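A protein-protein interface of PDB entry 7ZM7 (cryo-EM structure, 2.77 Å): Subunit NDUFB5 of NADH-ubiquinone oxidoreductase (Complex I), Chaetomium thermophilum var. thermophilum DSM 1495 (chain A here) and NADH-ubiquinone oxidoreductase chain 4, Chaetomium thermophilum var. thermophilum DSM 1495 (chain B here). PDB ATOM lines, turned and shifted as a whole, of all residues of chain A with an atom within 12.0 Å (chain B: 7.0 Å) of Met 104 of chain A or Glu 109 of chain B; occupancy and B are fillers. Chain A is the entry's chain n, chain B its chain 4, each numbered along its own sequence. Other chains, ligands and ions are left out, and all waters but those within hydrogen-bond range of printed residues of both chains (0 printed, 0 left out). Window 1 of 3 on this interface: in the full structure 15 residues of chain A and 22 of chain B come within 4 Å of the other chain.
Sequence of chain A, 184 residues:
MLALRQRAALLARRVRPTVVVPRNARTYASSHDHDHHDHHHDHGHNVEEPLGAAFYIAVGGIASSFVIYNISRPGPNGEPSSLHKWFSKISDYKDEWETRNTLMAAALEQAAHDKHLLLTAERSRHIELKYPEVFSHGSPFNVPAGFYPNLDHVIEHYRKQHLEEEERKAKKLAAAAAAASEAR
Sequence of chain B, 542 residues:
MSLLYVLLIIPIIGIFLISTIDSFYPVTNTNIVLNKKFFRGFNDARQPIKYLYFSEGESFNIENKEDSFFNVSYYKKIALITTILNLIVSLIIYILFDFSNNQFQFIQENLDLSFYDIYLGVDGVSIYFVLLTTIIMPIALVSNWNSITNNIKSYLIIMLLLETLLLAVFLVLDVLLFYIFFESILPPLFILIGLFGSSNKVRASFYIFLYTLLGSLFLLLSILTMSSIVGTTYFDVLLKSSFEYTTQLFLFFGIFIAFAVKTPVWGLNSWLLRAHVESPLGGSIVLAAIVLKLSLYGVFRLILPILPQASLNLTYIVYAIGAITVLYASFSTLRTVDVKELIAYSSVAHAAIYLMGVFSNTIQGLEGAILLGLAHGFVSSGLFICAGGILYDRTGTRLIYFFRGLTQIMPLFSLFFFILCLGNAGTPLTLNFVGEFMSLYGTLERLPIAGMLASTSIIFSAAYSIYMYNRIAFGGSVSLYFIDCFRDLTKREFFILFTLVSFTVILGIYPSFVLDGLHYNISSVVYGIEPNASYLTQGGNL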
ATOM      1  N   ASP A  95      21.623 -24.677  -2.887  1.00  0.00           N
ATOM      2  CA  ASP A  95      21.023 -24.941  -4.187  1.00  0.00           C
ATOM      3  C   ASP A  95      19.509 -24.798  -4.129  1.00  0.00           C
ATOM      4  O   ASP A  95      18.818 -25.193  -5.067  1.00  0.00           O
ATOM      5  CB  ASP A  95      21.407 -26.339  -4.682  1.00  0.00           C
ATOM      6  CG  ASP A  95      21.169 -27.408  -3.640  1.00  0.00           C
ATOM      7  OD1 ASP A  95      20.823 -27.053  -2.495  1.00  0.00           O
ATOM      8  OD2 ASP A  95      21.329 -28.603  -3.963  1.00  0.00           O
ATOM      9  N   GLU A  96      18.982 -24.235  -3.048  1.00  0.00           N
ATOM     10  CA  GLU A  96      17.539 -24.187  -2.867  1.00  0.00           C
ATOM     11  C   GLU A  96      16.871 -23.236  -3.843  1.00  0.00           C
ATOM     12  O   GLU A  96      15.742 -23.490  -4.264  1.00  0.00           O
ATOM     13  CB  GLU A  96      17.216 -23.811  -1.426  1.00  0.00           C
ATOM     14  CG  GLU A  96      15.744 -23.815  -1.092  1.00  0.00           C
ATOM     15  CD  GLU A  96      15.183 -22.419  -1.040  1.00  0.00           C
ATOM     16  OE1 GLU A  96      15.958 -21.490  -0.743  1.00  0.00           O
ATOM     17  OE2 GLU A  96      13.979 -22.243  -1.292  1.00  0.00           O
ATOM     18  N   TRP A  97      17.530 -22.145  -4.215  1.00  0.00           N
ATOM     19  CA  TRP A  97      16.914 -21.284  -5.253  1.00  0.00           C
ATOM     20  C   TRP A  97      17.045 -21.965  -6.618  1.00  0.00           C
ATOM     21  O   TRP A  97      16.071 -21.943  -7.383  1.00  0.00           O
ATOM     22  CB  TRP A  97      17.501 -19.869  -5.253  1.00  0.00           C
ATOM     23  CG  TRP A  97      17.456 -19.150  -3.940  1.00  0.00           C
ATOM     24  CD1 TRP A  97      18.490 -18.492  -3.342  1.00  0.00           C
ATOM     25  CD2 TRP A  97      16.325 -19.001  -3.061  1.00  0.00           C
ATOM     26  NE1 TRP A  97      18.084 -17.946  -2.155  1.00  0.00           N
ATOM     27  CE2 TRP A  97      16.763 -18.245  -1.954  1.00  0.00           C
ATOM     28  CE3 TRP A  97      14.994 -19.429  -3.096  1.00  0.00           C
ATOM     29  CZ2 TRP A  97      15.920 -17.917  -0.895  1.00  0.00           C
ATOM     30  CZ3 TRP A  97      14.162 -19.106  -2.048  1.00  0.00           C
ATOM     31  CH2 TRP A  97      14.623 -18.368  -0.960  1.00  0.00           C
ATOM     32  N   GLU A  98      18.196 -22.580  -6.887  1.00  0.00           N
ATOM     33  CA  GLU A  98      18.388 -23.211  -8.184  1.00  0.00           C
ATOM     34  C   GLU A  98      17.465 -24.402  -8.373  1.00  0.00           C
ATOM     35  O   GLU A  98      16.993 -24.650  -9.486  1.00  0.00           O
ATOM     36  CB  GLU A  98      19.844 -23.617  -8.361  1.00  0.00           C
ATOM     37  CG  GLU A  98      20.167 -24.065  -9.760  1.00  0.00           C
ATOM     38  CD  GLU A  98      19.819 -25.520  -9.984  1.00  0.00           C
ATOM     39  OE1 GLU A  98      19.862 -26.309  -9.015  1.00  0.00           O
ATOM     40  OE2 GLU A  98      19.411 -25.853 -11.107  1.00  0.00           O
ATOM     41  N   THR A  99      17.199 -25.161  -7.315  1.00  0.00           N
ATOM     42  CA  THR A  99      16.310 -26.302  -7.476  1.00  0.00           C
ATOM     43  C   THR A  99      14.870 -25.865  -7.712  1.00  0.00           C
ATOM     44  O   THR A  99      14.146 -26.524  -8.454  1.00  0.00           O
ATOM     45  CB  THR A  99      16.411 -27.239  -6.267  1.00  0.00           C
ATOM     46  OG1 THR A  99      15.652 -28.429  -6.515  1.00  0.00           O
ATOM     47  CG2 THR A  99      15.880 -26.582  -5.008  1.00  0.00           C
ATOM     48  N   ARG A 100      14.446 -24.746  -7.136  1.00  0.00           N
ATOM     49  CA  ARG A 100      13.023 -24.312  -7.239  1.00  0.00           C
ATOM     50  C   ARG A 100      12.781 -23.598  -8.568  1.00  0.00           C
ATOM     51  O   ARG A 100      11.702 -23.780  -9.140  1.00  0.00           O
ATOM     52  CB  ARG A 100      12.617 -23.475  -6.023  1.00  0.00           C
ATOM     53  CG  ARG A 100      12.427 -24.274  -4.745  1.00  0.00           C
ATOM     54  CD  ARG A 100      11.829 -23.396  -3.667  1.00  0.00           C
ATOM     55  NE  ARG A 100      11.603 -24.122  -2.426  1.00  0.00           N
ATOM     56  CZ  ARG A 100      11.100 -23.581  -1.325  1.00  0.00           C
ATOM     57  NH1 ARG A 100      10.772 -22.301  -1.309  1.00  0.00           N
ATOM     58  NH2 ARG A 100      10.932 -24.318  -0.242  1.00  0.00           N
ATOM     59  N   ASN A 101      13.751 -22.806  -9.018  1.00  0.00           N
ATOM     60  CA  ASN A 101      13.612 -22.027 -10.272  1.00  0.00           C
ATOM     61  C   ASN A 101      13.703 -22.960 -11.468  1.00  0.00           C
ATOM     62  O   ASN A 101      13.062 -22.663 -12.482  1.00  0.00           O
ATOM     63  CB  ASN A 101      14.710 -20.974 -10.415  1.00  0.00           C
ATOM     64  CG  ASN A 101      14.477 -19.721  -9.601  1.00  0.00           C
ATOM     65  OD1 ASN A 101      13.491 -19.021  -9.800  1.00  0.00           O
ATOM     66  ND2 ASN A 101      15.398 -19.416  -8.707  1.00  0.00           N
ATOM     67  N   THR A 102      14.490 -24.027 -11.346  1.00  0.00           N
ATOM     68  CA  THR A 102      14.621 -25.005 -12.456  1.00  0.00           C
ATOM     69  C   THR A 102      13.289 -25.710 -12.713  1.00  0.00           C
ATOM     70  O   THR A 102      12.926 -25.883 -13.885  1.00  0.00           O
ATOM     71  CB  THR A 102      15.750 -26.002 -12.179  1.00  0.00           C
ATOM     72  OG1 THR A 102      16.147 -26.585 -13.420  1.00  0.00           O
ATOM     73  CG2 THR A 102      15.354 -27.086 -11.200  1.00  0.00           C
ATOM     74  N   LEU A 103      12.584 -26.081 -11.650  1.00  0.00           N
ATOM     75  CA  LEU A 103      11.272 -26.739 -11.809  1.00  0.00           C
ATOM     76  C   LEU A 103      10.296 -25.768 -12.462  1.00  0.00           C
ATOM     77  O   LEU A 103       9.592 -26.191 -13.389  1.00  0.00           O
ATOM     78  CB  LEU A 103      10.793 -27.186 -10.430  1.00  0.00           C
ATOM     79  CG  LEU A 103      11.687 -28.200  -9.720  1.00  0.00           C
ATOM     80  CD1 LEU A 103      11.080 -28.612  -8.390  1.00  0.00           C
ATOM     81  CD2 LEU A 103      11.921 -29.418 -10.599  1.00  0.00           C
ATOM     82  N   MET A 104      10.265 -24.510 -12.025  1.00  0.00           N
ATOM     83  CA  MET A 104       9.277 -23.569 -12.530  1.00  0.00           C
ATOM     84  C   MET A 104       9.526 -23.243 -13.989  1.00  0.00           C
ATOM     85  O   MET A 104       8.584 -23.127 -14.775  1.00  0.00           O
ATOM     86  CB  MET A 104       9.312 -22.296 -11.696  1.00  0.00           C
ATOM     87  CG  MET A 104       8.125 -21.415 -11.896  1.00  0.00           C
ATOM     88  SD  MET A 104       6.657 -22.320 -11.429  1.00  0.00           S
ATOM     89  CE  MET A 104       7.169 -22.900  -9.812  1.00  0.00           C
ATOM     90  N   ALA A 105      10.792 -23.077 -14.356  1.00  0.00           N
ATOM     91  CA  ALA A 105      11.140 -22.832 -15.746  1.00  0.00           C
ATOM     92  C   ALA A 105      10.716 -23.993 -16.634  1.00  0.00           C
ATOM     93  O   ALA A 105      10.255 -23.784 -17.754  1.00  0.00           O
ATOM     94  CB  ALA A 105      12.638 -22.582 -15.858  1.00  0.00           C
ATOM     95  N   ALA A 106      10.860 -25.220 -16.150  1.00  0.00           N
ATOM     96  CA  ALA A 106      10.440 -26.378 -16.922  1.00  0.00           C
ATOM     97  C   ALA A 106       8.943 -26.353 -17.213  1.00  0.00           C
ATOM     98  O   ALA A 106       8.521 -26.611 -18.342  1.00  0.00           O
ATOM     99  CB  ALA A 106      10.814 -27.654 -16.176  1.00  0.00           C
ATOM    100  N   ALA A 107       8.130 -26.050 -16.203  1.00  0.00           N
ATOM    101  CA  ALA A 107       6.684 -26.063 -16.362  1.00  0.00           C
ATOM    102  C   ALA A 107       6.205 -24.897 -17.205  1.00  0.00           C
ATOM    103  O   ALA A 107       5.248 -25.030 -17.971  1.00  0.00           O
ATOM    104  CB  ALA A 107       6.020 -26.036 -14.994  1.00  0.00           C
ATOM    105  N   LEU A 108       6.829 -23.740 -17.064  1.00  0.00           N
ATOM    106  CA  LEU A 108       6.398 -22.612 -17.867  1.00  0.00           C
ATOM    107  C   LEU A 108       6.907 -22.716 -19.298  1.00  0.00           C
ATOM    108  O   LEU A 108       6.268 -22.180 -20.207  1.00  0.00           O
ATOM    109  CB  LEU A 108       6.815 -21.314 -17.184  1.00  0.00           C
ATOM    110  CG  LEU A 108       5.918 -21.065 -15.962  1.00  0.00           C
ATOM    111  CD1 LEU A 108       6.587 -20.208 -14.922  1.00  0.00           C
ATOM    112  CD2 LEU A 108       4.587 -20.462 -16.353  1.00  0.00           C
ATOM    113  N   GLU A 109       8.024 -23.415 -19.528  1.00  0.00           N
ATOM    114  CA  GLU A 109       8.347 -23.864 -20.881  1.00  0.00           C
ATOM    115  C   GLU A 109       7.317 -24.852 -21.411  1.00  0.00           C
ATOM    116  O   GLU A 109       7.028 -24.867 -22.611  1.00  0.00           O
ATOM    117  CB  GLU A 109       9.730 -24.507 -20.941  1.00  0.00           C
ATOM    118  CG  GLU A 109      10.912 -23.638 -20.602  1.00  0.00           C
ATOM    119  CD  GLU A 109      11.325 -22.751 -21.755  1.00  0.00           C
ATOM    120  OE1 GLU A 109      12.073 -21.778 -21.526  1.00  0.00           O
ATOM    121  OE2 GLU A 109      10.903 -23.032 -22.892  1.00  0.00           O
ATOM    122  N   GLN A 110       6.786 -25.711 -20.544  1.00  0.00           N
ATOM    123  CA  GLN A 110       5.861 -26.739 -21.001  1.00  0.00           C
ATOM    124  C   GLN A 110       4.536 -26.131 -21.440  1.00  0.00           C
ATOM    125  O   GLN A 110       3.927 -26.589 -22.411  1.00  0.00           O
ATOM    126  CB  GLN A 110       5.636 -27.763 -19.899  1.00  0.00           C
ATOM    127  CG  GLN A 110       4.749 -28.921 -20.294  1.00  0.00           C
ATOM    128  CD  GLN A 110       5.332 -29.745 -21.424  1.00  0.00           C
ATOM    129  OE1 GLN A 110       4.890 -29.657 -22.568  1.00  0.00           O
ATOM    130  NE2 GLN A 110       6.331 -30.555 -21.104  1.00  0.00           N
ATOM    131  N   ALA A 111       4.072 -25.103 -20.731  1.00  0.00           N
ATOM    132  CA  ALA A 111       2.817 -24.470 -21.093  1.00  0.00           C
ATOM    133  C   ALA A 111       2.998 -23.454 -22.206  1.00  0.00           C
ATOM    134  O   ALA A 111       2.019 -23.054 -22.840  1.00  0.00           O
ATOM    135  CB  ALA A 111       2.188 -23.825 -19.868  1.00  0.00           C
ATOM    136  N   ALA A 112       4.221 -22.991 -22.436  1.00  0.00           N
ATOM    137  CA  ALA A 112       4.493 -22.245 -23.657  1.00  0.00           C
ATOM    138  C   ALA A 112       4.273 -23.125 -24.877  1.00  0.00           C
ATOM    139  O   ALA A 112       3.708 -22.684 -25.882  1.00  0.00           O
ATOM    140  CB  ALA A 112       5.917 -21.704 -23.637  1.00  0.00           C
ATOM    141  N   HIS A 113       4.679 -24.392 -24.784  1.00  0.00           N
ATOM    142  CA  HIS A 113       4.486 -25.339 -25.911  1.00  0.00           C
ATOM    143  C   HIS A 113       3.010 -25.715 -26.013  1.00  0.00           C
ATOM    144  O   HIS A 113       2.505 -25.795 -27.154  1.00  0.00           O
ATOM    145  CB  HIS A 113       5.357 -26.588 -25.717  1.00  0.00           C
ATOM    146  CG  HIS A 113       4.771 -27.820 -26.317  1.00  0.00           C
ATOM    147  ND1 HIS A 113       4.782 -28.059 -27.675  1.00  0.00           N
ATOM    148  CD2 HIS A 113       4.148 -28.878 -25.751  1.00  0.00           C
ATOM    149  CE1 HIS A 113       4.192 -29.211 -27.920  1.00  0.00           C
ATOM    150  NE2 HIS A 113       3.793 -29.733 -26.757  1.00  0.00           N
ATOM    151  N   ILE B 107      11.966 -17.086  -4.058  1.00  0.00           N
ATOM    152  CA  ILE B 107      10.857 -17.568  -4.920  1.00  0.00           C
ATOM    153  C   ILE B 107      10.096 -18.684  -4.202  1.00  0.00           C
ATOM    154  O   ILE B 107      10.683 -19.353  -3.334  1.00  0.00           O
ATOM    155  CB  ILE B 107      11.400 -18.010  -6.292  1.00  0.00           C
ATOM    156  CG1 ILE B 107      12.078 -19.380  -6.243  1.00  0.00           C
ATOM    157  CG2 ILE B 107      12.310 -16.950  -6.885  1.00  0.00           C
ATOM    158  CD1 ILE B 107      11.551 -20.333  -7.283  1.00  0.00           C
ATOM    159  N   GLN B 108       8.819 -18.843  -4.534  1.00  0.00           N
ATOM    160  CA  GLN B 108       8.028 -19.954  -3.960  1.00  0.00           C
ATOM    161  C   GLN B 108       7.625 -20.844  -5.131  1.00  0.00           C
ATOM    162  O   GLN B 108       7.188 -20.300  -6.155  1.00  0.00           O
ATOM    163  CB  GLN B 108       6.790 -19.426  -3.232  1.00  0.00           C
ATOM    164  CG  GLN B 108       6.167 -20.446  -2.289  1.00  0.00           C
ATOM    165  CD  GLN B 108       4.988 -19.884  -1.534  1.00  0.00           C
ATOM    166  OE1 GLN B 108       4.591 -18.739  -1.727  1.00  0.00           O
ATOM    167  NE2 GLN B 108       4.416 -20.696  -0.661  1.00  0.00           N
ATOM    168  N   GLU B 109       7.770 -22.157  -4.976  1.00  0.00           N
ATOM    169  CA  GLU B 109       7.441 -23.082  -6.084  1.00  0.00           C
ATOM    170  C   GLU B 109       5.923 -23.227  -6.111  1.00  0.00           C
ATOM    171  O   GLU B 109       5.358 -23.716  -5.116  1.00  0.00           O
ATOM    172  CB  GLU B 109       8.110 -24.439  -5.874  1.00  0.00           C
ATOM    173  CG  GLU B 109       7.858 -25.409  -7.014  1.00  0.00           C
ATOM    174  CD  GLU B 109       8.207 -26.859  -6.724  1.00  0.00           C
ATOM    175  OE1 GLU B 109       8.752 -27.129  -5.636  1.00  0.00           O
ATOM    176  OE2 GLU B 109       7.924 -27.714  -7.586  1.00  0.00           O
ATOM    177  N   ASN B 110       5.296 -22.797  -7.202  1.00  0.00           N
ATOM    178  CA  ASN B 110       3.846 -22.803  -7.311  1.00  0.00           C
ATOM    179  C   ASN B 110       3.311 -24.123  -7.855  1.00  0.00           C
ATOM    180  O   ASN B 110       2.387 -24.701  -7.276  1.00  0.00           O
ATOM    181  CB  ASN B 110       3.376 -21.649  -8.194  1.00  0.00           C
ATOM    182  CG  ASN B 110       1.884 -21.422  -8.096  1.00  0.00           C
ATOM    183  OD1 ASN B 110       1.263 -21.740  -7.084  1.00  0.00           O
ATOM    184  ND2 ASN B 110       1.298 -20.876  -9.153  1.00  0.00           N
ATOM    185  N   LEU B 111       3.853 -24.583  -8.986  1.00  0.00           N
ATOM    186  CA  LEU B 111       3.486 -25.848  -9.635  1.00  0.00           C
ATOM    187  C   LEU B 111       1.973 -26.057  -9.716  1.00  0.00           C
ATOM    188  O   LEU B 111       1.500 -27.195  -9.793  1.00  0.00           O
ATOM    189  CB  LEU B 111       4.155 -27.066  -8.973  1.00  0.00           C
ATOM    190  CG  LEU B 111       3.807 -27.685  -7.612  1.00  0.00           C
ATOM    191  CD1 LEU B 111       4.429 -29.063  -7.542  1.00  0.00           C
ATOM    192  CD2 LEU B 111       4.340 -26.874  -6.452  1.00  0.00           C
ATOM    193  N   ASP B 112       1.199 -24.977  -9.705  1.00  0.00           N
ATOM    194  CA  ASP B 112      -0.250 -25.021  -9.888  1.00  0.00           C
ATOM    195  C   ASP B 112      -0.566 -23.985 -10.958  1.00  0.00           C
ATOM    196  O   ASP B 112      -0.901 -22.838 -10.654  1.00  0.00           O
ATOM    197  CB  ASP B 112      -0.992 -24.741  -8.584  1.00  0.00           C
ATOM    198  N   LEU B 113      -0.257 -24.240 -12.169  1.00  0.00           N
ATOM    199  CA  LEU B 113      -0.325 -23.212 -13.238  1.00  0.00           C
ATOM    200  C   LEU B 113      -1.746 -22.816 -13.620  1.00  0.00           C
ATOM    201  O   LEU B 113      -2.624 -23.697 -13.658  1.00  0.00           O
ATOM    202  CB  LEU B 113       0.441 -23.717 -14.464  1.00  0.00           C
ATOM    203  CG  LEU B 113       1.883 -23.226 -14.598  1.00  0.00           C
ATOM    204  CD1 LEU B 113       2.747 -23.725 -13.450  1.00  0.00           C
ATOM    205  CD2 LEU B 113       2.475 -23.660 -15.930  1.00  0.00           C
ATOM    206  N   TYR B 119       4.083 -14.539  -9.788  1.00  0.00           N
ATOM    207  CA  TYR B 119       5.391 -15.093  -9.488  1.00  0.00           C
ATOM    208  C   TYR B 119       6.241 -13.983  -8.903  1.00  0.00           C
ATOM    209  O   TYR B 119       6.512 -12.991  -9.582  1.00  0.00           O
ATOM    210  CB  TYR B 119       6.053 -15.655 -10.740  1.00  0.00           C
ATOM    211  CG  TYR B 119       5.432 -16.918 -11.250  1.00  0.00           C
ATOM    212  CD1 TYR B 119       5.843 -18.140 -10.768  1.00  0.00           C
ATOM    213  CD2 TYR B 119       4.433 -16.894 -12.207  1.00  0.00           C
ATOM    214  CE1 TYR B 119       5.287 -19.300 -11.225  1.00  0.00           C
ATOM    215  CE2 TYR B 119       3.864 -18.049 -12.664  1.00  0.00           C
ATOM    216  CZ  TYR B 119       4.302 -19.255 -12.171  1.00  0.00           C
ATOM    217  OH  TYR B 119       3.762 -20.442 -12.602  1.00  0.00           O
ATOM    218  N   TYR B 234       6.918 -15.186 -18.610  1.00  0.00           N
ATOM    219  CA  TYR B 234       7.824 -15.496 -17.517  1.00  0.00           C
ATOM    220  C   TYR B 234       9.258 -15.207 -17.929  1.00  0.00           C
ATOM    221  O   TYR B 234       9.693 -15.626 -18.999  1.00  0.00           O
ATOM    222  CB  TYR B 234       7.646 -16.968 -17.150  1.00  0.00           C
ATOM    223  CG  TYR B 234       8.436 -17.468 -15.977  1.00  0.00           C
ATOM    224  CD1 TYR B 234       8.111 -17.101 -14.681  1.00  0.00           C
ATOM    225  CD2 TYR B 234       9.486 -18.344 -16.168  1.00  0.00           C
ATOM    226  CE1 TYR B 234       8.826 -17.572 -13.624  1.00  0.00           C
ATOM    227  CE2 TYR B 234      10.197 -18.815 -15.128  1.00  0.00           C
ATOM    228  CZ  TYR B 234       9.873 -18.436 -13.858  1.00  0.00           C
ATOM    229  OH  TYR B 234      10.607 -18.931 -12.815  1.00  0.00           O
ATOM    230  N   ASP B 236      12.322 -16.177 -17.265  1.00  0.00           N
ATOM    231  CA  ASP B 236      13.304 -17.200 -17.609  1.00  0.00           C
ATOM    232  C   ASP B 236      13.109 -17.764 -19.005  1.00  0.00           C
ATOM    233  O   ASP B 236      14.076 -18.218 -19.615  1.00  0.00           O
ATOM    234  CB  ASP B 236      13.262 -18.330 -16.600  1.00  0.00           C
ATOM    235  CG  ASP B 236      13.924 -17.966 -15.307  1.00  0.00           C
ATOM    236  OD1 ASP B 236      14.851 -17.130 -15.335  1.00  0.00           O
ATOM    237  OD2 ASP B 236      13.524 -18.515 -14.259  1.00  0.00           O
ATOM    238  N   VAL B 237      11.889 -17.751 -19.525  1.00  0.00           N
ATOM    239  CA  VAL B 237      11.657 -18.287 -20.855  1.00  0.00           C
ATOM    240  C   VAL B 237      11.867 -17.221 -21.927  1.00  0.00           C
ATOM    241  O   VAL B 237      12.288 -17.545 -23.037  1.00  0.00           O
ATOM    242  CB  VAL B 237      10.249 -18.902 -20.923  1.00  0.00           C
ATOM    243  CG1 VAL B 237       9.937 -19.417 -22.317  1.00  0.00           C
ATOM    244  CG2 VAL B 237      10.085 -19.984 -19.891  1.00  0.00           C
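Hydrophobic or aromatic side chains of chain B that line the printed part of chain A: Ile 107, Leu 113, Tyr 119, Tyr 234 and Val 237. Of the 19 printed residues of chain A, 9 touch a printed residue of chain B. Hydrophobic or aromatic side chains of chain A within 4 Å of the printed part of chain B: Trp 97, Leu 103, Met 104, Leu 108 and Ala 111. Among the printed residues, no Asp or Glu carboxylate lies within 4 Å of a Lys or Arg side-chain nitrogen of the other chain.
CZ3 of Trp 97 of chain A touches N of Ile 107 of chain B (3.6 Å). Arg 100 of chain A touches Ile 107 of chain B. OD1 of Asn 101 of chain A touches CD1 of Ile 107 of chain B (3.4 Å). Met 104 of chain A touches Glu 109 of chain B (CE to CA, 3.7 Å). Asn 110 of chain B touches Met 104 of chain A. Met 104 of chain A touches Leu 111 of chain B. Met 104 of chain A touches Tyr 234 of chain B. Ala 107 of chain A touches Leu 113 of chain B (O to CD2, 3.7 Å). CD1 of Leu 108 of chain A touches CD1 of Tyr 234 of chain B (3.5 Å). Ala 111 of chain A touches Leu 113 of chain B.
Met 104 of chain A touches just these residues of chain B: Glu 109, Asn 110, Leu 111, Tyr 119 and Tyr 234. Printed residues of chain A within 4 Å of Glu 109 of chain B: Leu 103 (3.4 Å) and Met 104 (3.7 Å). Ile 107 of chain B touches just these residues of chain A: Trp 97 (3.6 Å), Arg 100 (3.5 Å) and Asn 101 (3.4 Å). Gln 108 of chain B touches none of the printed residues of chain A. Asn 110 of chain B touches one residue of chain A. Of chain A, only Met 104 comes within 4 Å of Leu 111 of chain B. No residue of chain A comes within 4 Å of Asp 112 of chain B. Of the printed residues of chain A, Tyr 119 of chain B touches Met 104 and Leu 108. Of the printed residues of chain A, Val 237 of chain B touches Glu 109 (3.1 Å). Of the printed residues of chain B, Arg 100 of chain A touches Ile 107. Of the printed residues of chain B, Leu 103 of chain A touches Glu 109 (3.4 Å). The nearest printed residue of chain B that does not touch Trp 97 of chain A is Gln 108 of chain B (5.9 Å).
The side-chain carboxylate of Asp 236 of chain B sits at hydrogen-bond distance from the side-chain hydroxyl of Tyr 234 of chain B (3.3 Å). ND2 of Asn 101 of chain A sits at hydrogen-bond distance from O of Trp 97 of chain A, 2.9 Å away. O of Asp 112 of chain B sits at hydrogen-bond distance from ND2 of Asn 110 of chain B (3.3 Å). OE2 of Glu 96 of chain A lies within salt-bridge range of NH1 of Arg 100 of chain A (3.2 Å).
The side-chain sulfur (SD) of Met 104 of chain A lies close to the side-chain hydroxyl (OH) of Tyr 119 of chain B (3.6 Å).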
